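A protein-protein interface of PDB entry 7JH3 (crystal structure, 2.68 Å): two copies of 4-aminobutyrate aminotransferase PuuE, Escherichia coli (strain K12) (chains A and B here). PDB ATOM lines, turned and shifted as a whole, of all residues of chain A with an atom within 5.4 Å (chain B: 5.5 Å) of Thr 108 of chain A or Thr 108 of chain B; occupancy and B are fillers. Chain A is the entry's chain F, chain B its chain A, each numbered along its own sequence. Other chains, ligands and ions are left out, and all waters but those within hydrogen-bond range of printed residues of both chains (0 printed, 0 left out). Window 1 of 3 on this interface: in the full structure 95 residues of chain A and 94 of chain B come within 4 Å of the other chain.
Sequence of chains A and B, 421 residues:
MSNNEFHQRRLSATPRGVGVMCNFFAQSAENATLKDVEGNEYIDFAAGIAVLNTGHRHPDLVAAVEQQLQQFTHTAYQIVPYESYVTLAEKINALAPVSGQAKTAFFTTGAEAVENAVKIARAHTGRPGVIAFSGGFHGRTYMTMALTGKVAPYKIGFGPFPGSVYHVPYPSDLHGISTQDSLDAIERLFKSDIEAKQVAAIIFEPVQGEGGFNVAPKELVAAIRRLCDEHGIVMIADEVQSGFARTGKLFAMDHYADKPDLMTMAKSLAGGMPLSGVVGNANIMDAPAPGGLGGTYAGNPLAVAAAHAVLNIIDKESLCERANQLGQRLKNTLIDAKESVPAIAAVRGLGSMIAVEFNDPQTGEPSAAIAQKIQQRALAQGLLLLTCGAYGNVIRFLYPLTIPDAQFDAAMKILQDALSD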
ATOM      1  N   PHE A 106     -22.533   5.948 -17.814  1.00  0.00           N
ATOM      2  CA  PHE A 106     -21.685   4.768 -17.754  1.00  0.00           C
ATOM      3  C   PHE A 106     -21.985   3.960 -16.504  1.00  0.00           C
ATOM      4  O   PHE A 106     -22.294   4.515 -15.447  1.00  0.00           O
ATOM      5  CB  PHE A 106     -20.202   5.145 -17.802  1.00  0.00           C
ATOM      6  CG  PHE A 106     -19.794   5.780 -19.096  1.00  0.00           C
ATOM      7  CD1 PHE A 106     -19.762   5.035 -20.263  1.00  0.00           C
ATOM      8  CD2 PHE A 106     -19.465   7.121 -19.152  1.00  0.00           C
ATOM      9  CE1 PHE A 106     -19.401   5.614 -21.458  1.00  0.00           C
ATOM     10  CE2 PHE A 106     -19.101   7.705 -20.349  1.00  0.00           C
ATOM     11  CZ  PHE A 106     -19.074   6.952 -21.502  1.00  0.00           C
ATOM     12  N   PHE A 107     -21.914   2.644 -16.655  1.00  0.00           N
ATOM     13  CA  PHE A 107     -22.092   1.703 -15.559  1.00  0.00           C
ATOM     14  C   PHE A 107     -20.945   0.703 -15.686  1.00  0.00           C
ATOM     15  O   PHE A 107     -19.915   0.969 -16.317  1.00  0.00           O
ATOM     16  CB  PHE A 107     -23.495   1.085 -15.611  1.00  0.00           C
ATOM     17  CG  PHE A 107     -24.596   2.109 -15.653  1.00  0.00           C
ATOM     18  CD1 PHE A 107     -25.058   2.699 -14.488  1.00  0.00           C
ATOM     19  CD2 PHE A 107     -25.152   2.502 -16.860  1.00  0.00           C
ATOM     20  CE1 PHE A 107     -26.064   3.654 -14.527  1.00  0.00           C
ATOM     21  CE2 PHE A 107     -26.157   3.453 -16.905  1.00  0.00           C
ATOM     22  CZ  PHE A 107     -26.612   4.030 -15.738  1.00  0.00           C
ATOM     23  N   THR A 108     -21.107  -0.481 -15.105  1.00  0.00           N
ATOM     24  CA  THR A 108     -19.993  -1.417 -15.015  1.00  0.00           C
ATOM     25  C   THR A 108     -20.168  -2.662 -15.873  1.00  0.00           C
ATOM     26  O   THR A 108     -19.253  -3.024 -16.620  1.00  0.00           O
ATOM     27  CB  THR A 108     -19.769  -1.804 -13.551  1.00  0.00           C
ATOM     28  OG1 THR A 108     -19.820  -0.621 -12.739  1.00  0.00           O
ATOM     29  CG2 THR A 108     -18.415  -2.465 -13.385  1.00  0.00           C
ATOM     30  N   THR A 109     -21.314  -3.334 -15.799  1.00  0.00           N
ATOM     31  CA  THR A 109     -21.559  -4.533 -16.587  1.00  0.00           C
ATOM     32  C   THR A 109     -22.614  -4.256 -17.648  1.00  0.00           C
ATOM     33  O   THR A 109     -23.460  -3.373 -17.490  1.00  0.00           O
ATOM     34  CB  THR A 109     -22.025  -5.699 -15.710  1.00  0.00           C
ATOM     35  OG1 THR A 109     -23.381  -5.472 -15.309  1.00  0.00           O
ATOM     36  CG2 THR A 109     -21.154  -5.822 -14.473  1.00  0.00           C
ATOM     37  N   GLY A 110     -22.557  -5.026 -18.737  1.00  0.00           N
ATOM     38  CA  GLY A 110     -23.560  -4.882 -19.781  1.00  0.00           C
ATOM     39  C   GLY A 110     -24.963  -5.173 -19.283  1.00  0.00           C
ATOM     40  O   GLY A 110     -25.936  -4.554 -19.729  1.00  0.00           O
ATOM     41  N   GLU A 112     -26.011  -4.390 -16.344  1.00  0.00           N
ATOM     42  CA  GLU A 112     -26.407  -3.122 -15.734  1.00  0.00           C
ATOM     43  C   GLU A 112     -26.819  -2.104 -16.790  1.00  0.00           C
ATOM     44  O   GLU A 112     -27.752  -1.323 -16.578  1.00  0.00           O
ATOM     45  CB  GLU A 112     -25.267  -2.560 -14.879  1.00  0.00           C
ATOM     46  CG  GLU A 112     -25.114  -3.202 -13.511  1.00  0.00           C
ATOM     47  CD  GLU A 112     -24.017  -2.552 -12.683  1.00  0.00           C
ATOM     48  OE1 GLU A 112     -23.101  -1.940 -13.279  1.00  0.00           O
ATOM     49  OE2 GLU A 112     -24.079  -2.649 -11.433  1.00  0.00           O
ATOM     50  N   PRO A 274     -13.583  -3.541 -17.111  1.00  0.00           N
ATOM     51  CA  PRO A 274     -15.021  -3.572 -16.810  1.00  0.00           C
ATOM     52  C   PRO A 274     -15.696  -2.209 -16.903  1.00  0.00           C
ATOM     53  O   PRO A 274     -15.586  -1.370 -16.003  1.00  0.00           O
ATOM     54  CB  PRO A 274     -15.069  -4.133 -15.384  1.00  0.00           C
ATOM     55  CG  PRO A 274     -13.727  -3.889 -14.831  1.00  0.00           C
ATOM     56  CD  PRO A 274     -12.752  -3.867 -15.943  1.00  0.00           C
ATOM     57  N   LEU A 275     -16.412  -1.995 -18.005  1.00  0.00           N
ATOM     58  CA  LEU A 275     -17.173  -0.775 -18.219  1.00  0.00           C
ATOM     59  C   LEU A 275     -18.372  -1.099 -19.098  1.00  0.00           C
ATOM     60  O   LEU A 275     -18.316  -1.998 -19.943  1.00  0.00           O
ATOM     61  CB  LEU A 275     -16.314   0.320 -18.867  1.00  0.00           C
ATOM     62  CG  LEU A 275     -16.950   1.694 -19.087  1.00  0.00           C
ATOM     63  CD1 LEU A 275     -17.262   2.365 -17.763  1.00  0.00           C
ATOM     64  CD2 LEU A 275     -16.042   2.568 -19.931  1.00  0.00           C
ATOM     65  N   SER A 276     -19.464  -0.373 -18.877  1.00  0.00           N
ATOM     66  CA  SER A 276     -20.620  -0.438 -19.752  1.00  0.00           C
ATOM     67  C   SER A 276     -21.223   0.953 -19.833  1.00  0.00           C
ATOM     68  O   SER A 276     -20.777   1.884 -19.160  1.00  0.00           O
ATOM     69  CB  SER A 276     -21.646  -1.461 -19.260  1.00  0.00           C
ATOM     70  OG  SER A 276     -22.285  -1.014 -18.082  1.00  0.00           O
ATOM     71  N   TYR A 297     -19.323   1.174  -8.627  1.00  0.00           N
ATOM     72  CA  TYR A 297     -18.190   1.070  -9.539  1.00  0.00           C
ATOM     73  C   TYR A 297     -18.403   1.805 -10.854  1.00  0.00           C
ATOM     74  O   TYR A 297     -17.451   1.909 -11.636  1.00  0.00           O
ATOM     75  CB  TYR A 297     -17.896  -0.399  -9.841  1.00  0.00           C
ATOM     76  CG  TYR A 297     -17.337  -1.182  -8.681  1.00  0.00           C
ATOM     77  CD1 TYR A 297     -16.402  -0.620  -7.819  1.00  0.00           C
ATOM     78  CD2 TYR A 297     -17.739  -2.491  -8.450  1.00  0.00           C
ATOM     79  CE1 TYR A 297     -15.882  -1.341  -6.759  1.00  0.00           C
ATOM     80  CE2 TYR A 297     -17.228  -3.220  -7.391  1.00  0.00           C
ATOM     81  CZ  TYR A 297     -16.301  -2.639  -6.552  1.00  0.00           C
ATOM     82  OH  TYR A 297     -15.793  -3.360  -5.500  1.00  0.00           O
ATOM     83  N   ALA A 298     -19.612   2.307 -11.109  1.00  0.00           N
ATOM     84  CA  ALA A 298     -19.980   2.814 -12.429  1.00  0.00           C
ATOM     85  C   ALA A 298     -18.992   3.860 -12.934  1.00  0.00           C
ATOM     86  O   ALA A 298     -18.574   4.756 -12.197  1.00  0.00           O
ATOM     87  CB  ALA A 298     -21.393   3.406 -12.385  1.00  0.00           C
ATOM     88  N   GLY A 299     -18.621   3.734 -14.207  1.00  0.00           N
ATOM     89  CA  GLY A 299     -17.695   4.661 -14.825  1.00  0.00           C
ATOM     90  C   GLY A 299     -16.309   4.590 -14.219  1.00  0.00           C
ATOM     91  O   GLY A 299     -15.719   5.620 -13.877  1.00  0.00           O
ATOM     92  N   PHE B 106     -17.264 -15.156  -7.859  1.00  0.00           N
ATOM     93  CA  PHE B 106     -16.968 -13.744  -8.041  1.00  0.00           C
ATOM     94  C   PHE B 106     -17.785 -13.170  -9.187  1.00  0.00           C
ATOM     95  O   PHE B 106     -18.046 -13.849 -10.186  1.00  0.00           O
ATOM     96  CB  PHE B 106     -15.476 -13.520  -8.294  1.00  0.00           C
ATOM     97  CG  PHE B 106     -14.619 -13.830  -7.107  1.00  0.00           C
ATOM     98  CD1 PHE B 106     -14.735 -13.084  -5.946  1.00  0.00           C
ATOM     99  CD2 PHE B 106     -13.707 -14.866  -7.143  1.00  0.00           C
ATOM    100  CE1 PHE B 106     -13.958 -13.366  -4.848  1.00  0.00           C
ATOM    101  CE2 PHE B 106     -12.928 -15.150  -6.047  1.00  0.00           C
ATOM    102  CZ  PHE B 106     -13.059 -14.400  -4.898  1.00  0.00           C
ATOM    103  N   PHE B 107     -18.188 -11.918  -9.024  1.00  0.00           N
ATOM    104  CA  PHE B 107     -18.873 -11.159 -10.060  1.00  0.00           C
ATOM    105  C   PHE B 107     -18.252  -9.766 -10.058  1.00  0.00           C
ATOM    106  O   PHE B 107     -17.129  -9.567  -9.583  1.00  0.00           O
ATOM    107  CB  PHE B 107     -20.391 -11.197  -9.826  1.00  0.00           C
ATOM    108  CG  PHE B 107     -20.928 -12.589  -9.614  1.00  0.00           C
ATOM    109  CD1 PHE B 107     -21.189 -13.418 -10.696  1.00  0.00           C
ATOM    110  CD2 PHE B 107     -21.148 -13.079  -8.335  1.00  0.00           C
ATOM    111  CE1 PHE B 107     -21.670 -14.697 -10.505  1.00  0.00           C
ATOM    112  CE2 PHE B 107     -21.629 -14.361  -8.138  1.00  0.00           C
ATOM    113  CZ  PHE B 107     -21.890 -15.167  -9.221  1.00  0.00           C
ATOM    114  N   THR B 108     -18.970  -8.775 -10.574  1.00  0.00           N
ATOM    115  CA  THR B 108     -18.363  -7.468 -10.791  1.00  0.00           C
ATOM    116  C   THR B 108     -18.892  -6.385  -9.862  1.00  0.00           C
ATOM    117  O   THR B 108     -18.095  -5.649  -9.275  1.00  0.00           O
ATOM    118  CB  THR B 108     -18.549  -7.049 -12.252  1.00  0.00           C
ATOM    119  OG1 THR B 108     -18.237  -8.160 -13.103  1.00  0.00           O
ATOM    120  CG2 THR B 108     -17.623  -5.894 -12.590  1.00  0.00           C
ATOM    121  N   THR B 109     -20.210  -6.262  -9.705  1.00  0.00           N
ATOM    122  CA  THR B 109     -20.796  -5.212  -8.882  1.00  0.00           C
ATOM    123  C   THR B 109     -21.528  -5.810  -7.687  1.00  0.00           C
ATOM    124  O   THR B 109     -21.914  -6.983  -7.690  1.00  0.00           O
ATOM    125  CB  THR B 109     -21.773  -4.343  -9.685  1.00  0.00           C
ATOM    126  OG1 THR B 109     -22.936  -5.113 -10.016  1.00  0.00           O
ATOM    127  CG2 THR B 109     -21.114  -3.841 -10.960  1.00  0.00           C
ATOM    128  N   GLY B 110     -21.723  -4.978  -6.660  1.00  0.00           N
ATOM    129  CA  GLY B 110     -22.413  -5.441  -5.468  1.00  0.00           C
ATOM    130  C   GLY B 110     -23.843  -5.859  -5.746  1.00  0.00           C
ATOM    131  O   GLY B 110     -24.308  -6.892  -5.252  1.00  0.00           O
ATOM    132  N   GLU B 112     -24.838  -7.052  -8.455  1.00  0.00           N
ATOM    133  CA  GLU B 112     -24.713  -8.338  -9.131  1.00  0.00           C
ATOM    134  C   GLU B 112     -24.536  -9.470  -8.124  1.00  0.00           C
ATOM    135  O   GLU B 112     -25.097 -10.561  -8.294  1.00  0.00           O
ATOM    136  CB  GLU B 112     -23.539  -8.282 -10.104  1.00  0.00           C
ATOM    137  CG  GLU B 112     -23.691  -9.126 -11.331  1.00  0.00           C
ATOM    138  CD  GLU B 112     -22.646  -8.792 -12.369  1.00  0.00           C
ATOM    139  OE1 GLU B 112     -21.451  -8.708 -12.005  1.00  0.00           O
ATOM    140  OE2 GLU B 112     -23.023  -8.596 -13.546  1.00  0.00           O
ATOM    141  N   PRO B 274     -13.207  -2.837  -9.540  1.00  0.00           N
ATOM    142  CA  PRO B 274     -14.552  -3.429  -9.651  1.00  0.00           C
ATOM    143  C   PRO B 274     -14.575  -4.947  -9.500  1.00  0.00           C
ATOM    144  O   PRO B 274     -14.225  -5.690 -10.422  1.00  0.00           O
ATOM    145  CB  PRO B 274     -15.019  -2.991 -11.046  1.00  0.00           C
ATOM    146  CG  PRO B 274     -13.789  -2.588 -11.769  1.00  0.00           C
ATOM    147  CD  PRO B 274     -12.766  -2.173 -10.777  1.00  0.00           C
ATOM    148  N   LEU B 275     -15.003  -5.411  -8.326  1.00  0.00           N
ATOM    149  CA  LEU B 275     -15.092  -6.831  -8.020  1.00  0.00           C
ATOM    150  C   LEU B 275     -16.139  -7.040  -6.936  1.00  0.00           C
ATOM    151  O   LEU B 275     -16.207  -6.271  -5.974  1.00  0.00           O
ATOM    152  CB  LEU B 275     -13.746  -7.395  -7.553  1.00  0.00           C
ATOM    153  CG  LEU B 275     -13.703  -8.884  -7.197  1.00  0.00           C
ATOM    154  CD1 LEU B 275     -13.874  -9.740  -8.446  1.00  0.00           C
ATOM    155  CD2 LEU B 275     -12.408  -9.226  -6.469  1.00  0.00           C
ATOM    156  N   SER B 276     -16.948  -8.081  -7.091  1.00  0.00           N
ATOM    157  CA  SER B 276     -17.884  -8.490  -6.056  1.00  0.00           C
ATOM    158  C   SER B 276     -17.806 -10.000  -5.889  1.00  0.00           C
ATOM    159  O   SER B 276     -17.121 -10.694  -6.643  1.00  0.00           O
ATOM    160  CB  SER B 276     -19.315  -8.058  -6.390  1.00  0.00           C
ATOM    161  OG  SER B 276     -19.783  -8.734  -7.541  1.00  0.00           O
ATOM    162  N   TYR B 297     -17.514  -9.788 -17.224  1.00  0.00           N
ATOM    163  CA  TYR B 297     -16.439  -9.181 -16.453  1.00  0.00           C
ATOM    164  C   TYR B 297     -16.167  -9.899 -15.139  1.00  0.00           C
ATOM    165  O   TYR B 297     -15.174  -9.576 -14.478  1.00  0.00           O
ATOM    166  CB  TYR B 297     -16.766  -7.714 -16.155  1.00  0.00           C
ATOM    167  CG  TYR B 297     -16.776  -6.800 -17.365  1.00  0.00           C
ATOM    168  CD1 TYR B 297     -15.868  -6.970 -18.403  1.00  0.00           C
ATOM    169  CD2 TYR B 297     -17.698  -5.766 -17.465  1.00  0.00           C
ATOM    170  CE1 TYR B 297     -15.877  -6.134 -19.508  1.00  0.00           C
ATOM    171  CE2 TYR B 297     -17.716  -4.926 -18.566  1.00  0.00           C
ATOM    172  CZ  TYR B 297     -16.803  -5.111 -19.583  1.00  0.00           C
ATOM    173  OH  TYR B 297     -16.820  -4.272 -20.678  1.00  0.00           O
ATOM    174  N   ALA B 298     -17.015 -10.854 -14.755  1.00  0.00           N
ATOM    175  CA  ALA B 298     -16.996 -11.410 -13.408  1.00  0.00           C
ATOM    176  C   ALA B 298     -15.611 -11.914 -13.022  1.00  0.00           C
ATOM    177  O   ALA B 298     -14.965 -12.647 -13.778  1.00  0.00           O
ATOM    178  CB  ALA B 298     -18.021 -12.541 -13.300  1.00  0.00           C
ATOM    179  N   GLY B 299     -15.162 -11.510 -11.835  1.00  0.00           N
ATOM    180  CA  GLY B 299     -13.856 -11.897 -11.336  1.00  0.00           C
ATOM    181  C   GLY B 299     -12.732 -11.353 -12.190  1.00  0.00           C
ATOM    182  O   GLY B 299     -11.806 -12.088 -12.549  1.00  0.00           O
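The backbone NH of Thr 108 of chain B lies within hydrogen-bond range of the side-chain carboxylate of Glu 112 of chain B (2.9 Å). OG1 of Thr 109 of chain B sits at hydrogen-bond distance from N of Glu 112 of chain B (3.1 Å). OG of Ser 276 of chain B lies within hydrogen-bond range of O of Thr 109 of chain B. N of Thr 108 of chain A sits at hydrogen-bond distance from OE1 of Glu 112 of chain A (3.1 Å). N of Glu 112 of chain A sits at hydrogen-bond distance from OG1 of Thr 109 of chain A (3.0 Å). O of Thr 109 of chain A sits at hydrogen-bond distance from OG of Ser 276 of chain A, at 2.7 Å.
Thr 108 of chain A touches its own counterpart, Thr 108 of chain B. Thr 108 of chain A touches Thr 109 of chain B, and with the chains exchanged Thr 109 of chain A touches Thr 108 of chain B. Pro 274 of chain A touches its own counterpart, Pro 274 of chain B. Pro 274 of chain A touches Tyr 297 of chain B, and with the chains exchanged Tyr 297 of chain A touches Pro 274 of chain B.
Thr 108 of chain B touches just these residues of chain A: Thr 108 (3.6 Å), Thr 109 (3.6 Å) and Tyr 297 (3.2 Å). Of the printed residues of chain A, Thr 109 of chain B touches Thr 108 and Glu 112. Printed residues of chain A within 4 Å of Leu 275 of chain B: Tyr 297. Phe 107 of chain B touches none of the printed residues of chain A. The nearest residue of chain A that does not touch Thr 108 of chain B is Pro 274 of chain A (4.2 Å).
OE2 of Glu 112 of chain A lies within hydrogen-bond range of OG1 of Thr 109 of chain B, at 3.1 Å. The backbone carbonyl oxygen of Leu 275 of chain B is in hydrogen-bond range of the side-chain hydroxyl of Tyr 297 of chain A (3.0 Å). The side-chain hydroxyl (OH) of Tyr 297 of chain B is in hydrogen-bond range of the backbone carbonyl oxygen (O) of Leu 275 of chain A (2.8 Å).
Among the printed residues, merely in contact across the chains: Thr 108 of chain A with Thr 108 of chain B (3.6 Å), Thr 108 of chain A with Thr 109 of chain B (3.6 Å), Thr 108 of chain A with Tyr 297 of chain B (3.1 Å), Thr 109 of chain A with Thr 108 of chain B (3.6 Å), Thr 109 of chain A with Glu 112 of chain B (3.5 Å), Pro 274 of chain A with Pro 274 of chain B (3.3 Å), Pro 274 of chain A with Tyr 297 of chain B (3.5 Å), Tyr 297 of chain A with Thr 108 of chain B (3.2 Å) and Tyr 297 of chain A with Pro 274 of chain B (3.5 Å).
Of the 12 printed residues of chain B, 6 touch a printed residue of chain A. Along chain B the printed residues that touch a printed residue of chain A span positions 108 to 297. Of the 12 printed residues of chain A, 6 touch a printed residue of chain B. Printed residues of chain A that touch a printed residue of chain B: Thr 108, Thr 109, Glu 112, Pro 274, Leu 275 and Tyr 297. Among the printed residues, no Asp or Glu carboxylate lies within 4 Å of a Lys or Arg side-chain nitrogen of the other chain.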
